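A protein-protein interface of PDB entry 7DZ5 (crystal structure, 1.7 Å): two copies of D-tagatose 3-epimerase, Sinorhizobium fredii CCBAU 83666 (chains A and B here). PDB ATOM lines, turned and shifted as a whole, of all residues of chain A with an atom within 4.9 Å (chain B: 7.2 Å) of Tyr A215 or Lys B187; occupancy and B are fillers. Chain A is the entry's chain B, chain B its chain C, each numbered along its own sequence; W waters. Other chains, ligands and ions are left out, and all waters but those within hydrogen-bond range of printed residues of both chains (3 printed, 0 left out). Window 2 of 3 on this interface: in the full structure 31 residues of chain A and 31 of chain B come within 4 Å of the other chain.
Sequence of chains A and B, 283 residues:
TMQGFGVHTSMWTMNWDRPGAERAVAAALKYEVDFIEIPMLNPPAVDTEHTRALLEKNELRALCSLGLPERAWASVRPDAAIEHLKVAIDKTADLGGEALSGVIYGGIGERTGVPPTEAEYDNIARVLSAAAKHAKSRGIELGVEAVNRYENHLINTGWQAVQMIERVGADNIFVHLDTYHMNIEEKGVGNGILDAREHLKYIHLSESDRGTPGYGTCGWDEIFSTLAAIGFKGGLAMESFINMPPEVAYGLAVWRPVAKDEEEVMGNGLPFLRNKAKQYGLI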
ATOM      1  N   GLU A 207      12.894   4.711   5.265  1.00  0.00           N
ATOM      2  CA  GLU A 207      13.570   4.850   6.547  1.00  0.00           C
ATOM      3  C   GLU A 207      12.820   5.844   7.440  1.00  0.00           C
ATOM      4  O   GLU A 207      12.010   6.667   6.989  1.00  0.00           O
ATOM      5  CB  GLU A 207      15.031   5.277   6.341  1.00  0.00           C
ATOM      6  CG  GLU A 207      15.934   5.109   7.559  1.00  0.00           C
ATOM      7  CD  GLU A 207      15.776   3.746   8.228  1.00  0.00           C
ATOM      8  OE1 GLU A 207      16.338   2.760   7.727  1.00  0.00           O
ATOM      9  OE2 GLU A 207      15.076   3.661   9.236  1.00  0.00           O
ATOM     10  N   ASP A 209      13.546   8.530   8.905  1.00  0.00           N
ATOM     11  CA  ASP A 209      13.730   9.954   8.642  1.00  0.00           C
ATOM     12  C   ASP A 209      13.508  10.292   7.175  1.00  0.00           C
ATOM     13  O   ASP A 209      13.875  11.394   6.726  1.00  0.00           O
ATOM     14  CB  ASP A 209      15.132  10.399   9.078  1.00  0.00           C
ATOM     15  CG  ASP A 209      16.249   9.722   8.294  1.00  0.00           C
ATOM     16  OD1 ASP A 209      15.989   8.759   7.533  1.00  0.00           O
ATOM     17  OD2 ASP A 209      17.424  10.159   8.425  1.00  0.00           O
ATOM     18  N   GLY A 211      15.124   9.107   4.789  1.00  0.00           N
ATOM     19  CA  GLY A 211      16.397   9.107   4.100  1.00  0.00           C
ATOM     20  C   GLY A 211      16.753   7.793   3.442  1.00  0.00           C
ATOM     21  O   GLY A 211      16.103   7.380   2.473  1.00  0.00           O
ATOM     22  N   THR A 212      17.791   7.128   3.959  1.00  0.00           N
ATOM     23  CA  THR A 212      18.342   5.933   3.325  1.00  0.00           C
ATOM     24  C   THR A 212      17.925   4.696   4.090  1.00  0.00           C
ATOM     25  O   THR A 212      18.378   4.511   5.227  1.00  0.00           O
ATOM     26  CB  THR A 212      19.865   6.017   3.287  1.00  0.00           C
ATOM     27  OG1 THR A 212      20.244   7.218   2.616  1.00  0.00           O
ATOM     28  CG2 THR A 212      20.465   4.823   2.559  1.00  0.00           C
ATOM     29  N   PRO A 213      17.128   3.805   3.511  1.00  0.00           N
ATOM     30  CA  PRO A 213      16.805   2.545   4.197  1.00  0.00           C
ATOM     31  C   PRO A 213      18.051   1.805   4.656  1.00  0.00           C
ATOM     32  O   PRO A 213      19.006   1.622   3.910  1.00  0.00           O
ATOM     33  CB  PRO A 213      16.037   1.756   3.131  1.00  0.00           C
ATOM     34  CG  PRO A 213      15.326   2.858   2.362  1.00  0.00           C
ATOM     35  CD  PRO A 213      16.370   3.954   2.263  1.00  0.00           C
ATOM     36  N   GLY A 214      18.017   1.355   5.906  1.00  0.00           N
ATOM     37  CA  GLY A 214      19.122   0.677   6.531  1.00  0.00           C
ATOM     38  C   GLY A 214      19.841   1.517   7.563  1.00  0.00           C
ATOM     39  O   GLY A 214      20.615   0.966   8.375  1.00  0.00           O
ATOM     40  N   TYR A 215      19.609   2.828   7.554  1.00  0.00           N
ATOM     41  CA  TYR A 215      20.407   3.794   8.302  1.00  0.00           C
ATOM     42  C   TYR A 215      19.446   4.747   9.009  1.00  0.00           C
ATOM     43  O   TYR A 215      19.347   5.932   8.699  1.00  0.00           O
ATOM     44  CB  TYR A 215      21.398   4.511   7.362  1.00  0.00           C
ATOM     45  CG  TYR A 215      22.216   3.473   6.632  1.00  0.00           C
ATOM     46  CD1 TYR A 215      21.740   2.858   5.473  1.00  0.00           C
ATOM     47  CD2 TYR A 215      23.415   3.026   7.155  1.00  0.00           C
ATOM     48  CE1 TYR A 215      22.461   1.845   4.842  1.00  0.00           C
ATOM     49  CE2 TYR A 215      24.137   2.036   6.537  1.00  0.00           C
ATOM     50  CZ  TYR A 215      23.661   1.447   5.378  1.00  0.00           C
ATOM     51  OH  TYR A 215      24.392   0.460   4.777  1.00  0.00           O
ATOM     52  N   GLY A 216      18.765   4.212  10.009  1.00  0.00           N
ATOM     53  CA  GLY A 216      17.809   4.981  10.784  1.00  0.00           C
ATOM     54  C   GLY A 216      17.345   4.204  11.997  1.00  0.00           C
ATOM     55  O   GLY A 216      18.152   3.552  12.672  1.00  0.00           O
ATOM     56  N   THR A 217      16.043   4.267  12.289  1.00  0.00           N
ATOM     57  CA  THR A 217      15.484   3.613  13.462  1.00  0.00           C
ATOM     58  C   THR A 217      14.388   2.592  13.166  1.00  0.00           C
ATOM     59  O   THR A 217      13.829   2.023  14.110  1.00  0.00           O
ATOM     60  CB  THR A 217      14.910   4.628  14.457  1.00  0.00           C
ATOM     61  OG1 THR A 217      13.678   5.123  13.948  1.00  0.00           O
ATOM     62  CG2 THR A 217      15.862   5.768  14.719  1.00  0.00           C
ATOM     63  N   VAL A 258      17.099  15.082   3.891  1.00  0.00           N
ATOM     64  CA  VAL A 258      16.912  13.750   4.480  1.00  0.00           C
ATOM     65  C   VAL A 258      18.116  12.838   4.298  1.00  0.00           C
ATOM     66  O   VAL A 258      18.190  11.790   4.957  1.00  0.00           O
ATOM     67  CB  VAL A 258      15.686  13.029   3.887  1.00  0.00           C
ATOM     68  CG1 VAL A 258      14.434  13.890   4.068  1.00  0.00           C
ATOM     69  CG2 VAL A 258      15.887  12.658   2.425  1.00  0.00           C
ATOM     70  N   ALA A 259      19.051  13.201   3.421  1.00  0.00           N
ATOM     71  CA  ALA A 259      20.193  12.375   3.054  1.00  0.00           C
ATOM     72  C   ALA A 259      21.142  13.244   2.231  1.00  0.00           C
ATOM     73  O   ALA A 259      20.798  14.354   1.828  1.00  0.00           O
ATOM     74  CB  ALA A 259      19.762  11.137   2.280  1.00  0.00           C
ATOM     75  N   ASN A 268      23.055   2.909  -1.391  1.00  0.00           N
ATOM     76  CA  ASN A 268      23.119   2.179  -0.130  1.00  0.00           C
ATOM     77  C   ASN A 268      21.776   1.550   0.237  1.00  0.00           C
ATOM     78  O   ASN A 268      21.741   0.422   0.731  1.00  0.00           O
ATOM     79  CB  ASN A 268      23.571   3.093   1.017  1.00  0.00           C
ATOM     80  CG  ASN A 268      24.970   3.641   0.813  1.00  0.00           C
ATOM     81  OD1 ASN A 268      25.701   3.155  -0.010  1.00  0.00           O
ATOM     82  ND2 ASN A 268      25.341   4.641   1.599  1.00  0.00           N
ATOM     83  N   THR B 157      16.664  18.162  16.111  1.00  0.00           N
ATOM     84  CA  THR B 157      17.725  17.222  16.413  1.00  0.00           C
ATOM     85  C   THR B 157      18.567  17.718  17.581  1.00  0.00           C
ATOM     86  O   THR B 157      18.593  18.913  17.902  1.00  0.00           O
ATOM     87  CB  THR B 157      18.652  17.049  15.213  1.00  0.00           C
ATOM     88  OG1 THR B 157      19.229  18.333  14.900  1.00  0.00           O
ATOM     89  CG2 THR B 157      17.888  16.514  14.014  1.00  0.00           C
ATOM     90  N   MET B 182      13.361  11.533  18.822  1.00  0.00           N
ATOM     91  CA  MET B 182      14.573  11.060  18.161  1.00  0.00           C
ATOM     92  C   MET B 182      14.291   9.861  17.260  1.00  0.00           C
ATOM     93  O   MET B 182      14.973   9.681  16.249  1.00  0.00           O
ATOM     94  CB  MET B 182      15.625  10.685  19.208  1.00  0.00           C
ATOM     95  CG  MET B 182      16.151  11.865  19.989  1.00  0.00           C
ATOM     96  SD  MET B 182      17.675  11.423  20.873  1.00  0.00           S
ATOM     97  CE  MET B 182      16.888  10.452  22.087  1.00  0.00           C
ATOM     98  N   ILE B 184      12.047   9.567  15.236  1.00  0.00           N
ATOM     99  CA  ILE B 184      11.734  10.132  13.921  1.00  0.00           C
ATOM    100  C   ILE B 184      12.911  10.915  13.346  1.00  0.00           C
ATOM    101  O   ILE B 184      13.266  10.756  12.181  1.00  0.00           O
ATOM    102  CB  ILE B 184      10.482  11.041  14.023  1.00  0.00           C
ATOM    103  CG1 ILE B 184       9.282  10.273  14.519  1.00  0.00           C
ATOM    104  CG2 ILE B 184      10.154  11.632  12.677  1.00  0.00           C
ATOM    105  CD1 ILE B 184       8.127  11.175  15.058  1.00  0.00           C
ATOM    106  N   GLU B 185      13.543  11.761  14.142  1.00  0.00           N
ATOM    107  CA  GLU B 185      14.452  12.769  13.621  1.00  0.00           C
ATOM    108  C   GLU B 185      15.912  12.342  13.514  1.00  0.00           C
ATOM    109  O   GLU B 185      16.629  12.885  12.653  1.00  0.00           O
ATOM    110  CB  GLU B 185      14.388  14.010  14.506  1.00  0.00           C
ATOM    111  CG  GLU B 185      13.012  14.621  14.515  1.00  0.00           C
ATOM    112  CD  GLU B 185      12.580  15.095  13.133  1.00  0.00           C
ATOM    113  OE1 GLU B 185      13.453  15.490  12.320  1.00  0.00           O
ATOM    114  OE2 GLU B 185      11.361  15.038  12.853  1.00  0.00           O
ATOM    115  N   GLU B 186      16.394  11.422  14.364  1.00  0.00           N
ATOM    116  CA  GLU B 186      17.825  11.123  14.420  1.00  0.00           C
ATOM    117  C   GLU B 186      18.173   9.964  13.496  1.00  0.00           C
ATOM    118  O   GLU B 186      17.480   8.942  13.458  1.00  0.00           O
ATOM    119  CB  GLU B 186      18.298  10.822  15.844  1.00  0.00           C
ATOM    120  CG  GLU B 186      17.953  11.902  16.855  1.00  0.00           C
ATOM    121  CD  GLU B 186      18.759  13.195  16.734  1.00  0.00           C
ATOM    122  OE1 GLU B 186      19.735  13.272  15.950  1.00  0.00           O
ATOM    123  OE2 GLU B 186      18.414  14.159  17.464  1.00  0.00           O
ATOM    124  N   LYS B 187      19.254  10.137  12.739  1.00  0.00           N
ATOM    125  CA  LYS B 187      19.679   9.153  11.754  1.00  0.00           C
ATOM    126  C   LYS B 187      20.457   8.088  12.513  1.00  0.00           C
ATOM    127  O   LYS B 187      21.688   8.028  12.496  1.00  0.00           O
ATOM    128  CB  LYS B 187      20.496   9.822  10.663  1.00  0.00           C
ATOM    129  CG  LYS B 187      20.655   8.963   9.415  1.00  0.00           C
ATOM    130  CD  LYS B 187      21.545   9.662   8.393  1.00  0.00           C
ATOM    131  CE  LYS B 187      20.804  10.779   7.644  1.00  0.00           C
ATOM    132  NZ  LYS B 187      19.743  10.280   6.705  1.00  0.00           N
ATOM    133  N   GLY B 188      19.709   7.231  13.196  1.00  0.00           N
ATOM    134  CA  GLY B 188      20.276   6.386  14.220  1.00  0.00           C
ATOM    135  C   GLY B 188      20.114   7.102  15.543  1.00  0.00           C
ATOM    136  O   GLY B 188      20.646   8.193  15.728  1.00  0.00           O
ATOM    137  N   VAL B 189      19.364   6.505  16.468  1.00  0.00           N
ATOM    138  CA  VAL B 189      18.941   7.248  17.654  1.00  0.00           C
ATOM    139  C   VAL B 189      20.147   7.684  18.476  1.00  0.00           C
ATOM    140  O   VAL B 189      20.164   8.779  19.039  1.00  0.00           O
ATOM    141  CB  VAL B 189      17.933   6.416  18.478  1.00  0.00           C
ATOM    142  CG1 VAL B 189      18.541   5.138  19.068  1.00  0.00           C
ATOM    143  CG2 VAL B 189      17.373   7.267  19.604  1.00  0.00           C
ATOM    144  N   GLY B 190      21.194   6.857  18.542  1.00  0.00           N
ATOM    145  CA  GLY B 190      22.356   7.239  19.336  1.00  0.00           C
ATOM    146  C   GLY B 190      23.016   8.533  18.876  1.00  0.00           C
ATOM    147  O   GLY B 190      23.692   9.203  19.666  1.00  0.00           O
ATOM    148  N   ASN B 191      22.877   8.880  17.598  1.00  0.00           N
ATOM    149  CA  ASN B 191      23.465  10.123  17.098  1.00  0.00           C
ATOM    150  C   ASN B 191      22.905  11.369  17.788  1.00  0.00           C
ATOM    151  O   ASN B 191      23.626  12.358  17.935  1.00  0.00           O
ATOM    152  CB  ASN B 191      23.276  10.242  15.582  1.00  0.00           C
ATOM    153  CG  ASN B 191      24.372   9.534  14.813  1.00  0.00           C
ATOM    154  OD1 ASN B 191      25.551   9.624  15.166  1.00  0.00           O
ATOM    155  ND2 ASN B 191      23.995   8.826  13.757  1.00  0.00           N
ATOM    156  N   GLY B 192      21.645  11.356  18.217  1.00  0.00           N
ATOM    157  CA  GLY B 192      21.129  12.506  18.940  1.00  0.00           C
ATOM    158  C   GLY B 192      21.823  12.685  20.272  1.00  0.00           C
ATOM    159  O   GLY B 192      22.180  13.803  20.659  1.00  0.00           O
ATOM    160  N   GLU B 222      20.422   0.543  22.255  1.00  0.00           N
ATOM    161  CA  GLU B 222      21.266   1.609  21.720  1.00  0.00           C
ATOM    162  C   GLU B 222      21.183   2.880  22.570  1.00  0.00           C
ATOM    163  O   GLU B 222      22.209   3.515  22.853  1.00  0.00           O
ATOM    164  CB  GLU B 222      20.853   1.898  20.280  1.00  0.00           C
ATOM    165  CG  GLU B 222      21.663   3.002  19.616  1.00  0.00           C
ATOM    166  CD  GLU B 222      21.282   3.249  18.168  1.00  0.00           C
ATOM    167  OE1 GLU B 222      20.488   2.478  17.588  1.00  0.00           O
ATOM    168  OE2 GLU B 222      21.788   4.239  17.603  1.00  0.00           O
HETATM  169  O   HOH W   1      18.842   3.650  15.765  1.00  0.00           O
HETATM  170  O   HOH W   2      18.464   7.656   6.705  1.00  0.00           O
HETATM  171  O   HOH W   3      21.073   8.855   4.565  1.00  0.00           O
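Of chain B, only Lys B187 comes within 4 Å of Tyr A215.
Printed residues of chain A within 4 Å of Lys B187: Asp A209 (2.9 Å), Tyr A215 (3.4 Å) and Val A258 (2.8 Å).
Gly A214 touches none of the printed residues of chain B.
Printed residues of chain B within 4 Å of Thr A217: Glu B186 and Val B189.
Of the printed residues of chain B, Gly A216 touches Gly B188 (3.8 Å).
The nearest residue of chain A that does not touch Lys B187 is Ala A259 (4.2 Å).
CB of Asp A209 touches O of Ile B184, 3.6 Å away.
Lys B187 touches Tyr A215 (CG to O, 3.4 Å).
CA of Gly A216 touches N of Gly B188, at 3.8 Å.
Glu B186 touches Thr A217.
Thr A217 touches Val B189.
Water W3 bridges OG1 of Thr A212 (2.7 Å) and NZ of Lys B187 (2.9 Å).
Water W1 lies within hydrogen-bond range of the side-chain carboxylate of Glu B222, the backbone NH of Val B189 and the backbone carbonyl oxygen of Gly A216.
Water W2 lies within hydrogen-bond range of O of Tyr A215 (2.8 Å), OD1 of Asp A209 (2.8 Å), N of Thr A212 (2.9 Å) and NZ of Lys B187 (2.9 Å).
OD2 of Asp A209 lies within salt-bridge range of NZ of Lys B187 (2.9 Å).
The side-chain amino group (NZ) of Lys B187 lies within hydrogen-bond range of the backbone carbonyl oxygen (O) of Val A258 (2.8 Å).
Of the 12 printed residues of chain A, 5 touch a printed residue of chain B.
Of the 12 printed residues of chain B, 5 touch a printed residue of chain A.
The side-chain carboxylate of Glu A207 lies within hydrogen-bond range of the backbone NH of Tyr A215, at 3.3 Å.
OD1 of Asp A209 lies within hydrogen-bond range of N of Gly A211, at 2.9 Å.
The backbone carbonyl oxygen (O) of Lys B187 lies within hydrogen-bond range of the side-chain amide nitrogen (ND2) of Asn B191 (2.7 Å).
The backbone NH of Thr A217 sits at hydrogen-bond distance from the side-chain carboxylate of Glu A207 (3.3 Å).
No position is printed for both chains.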
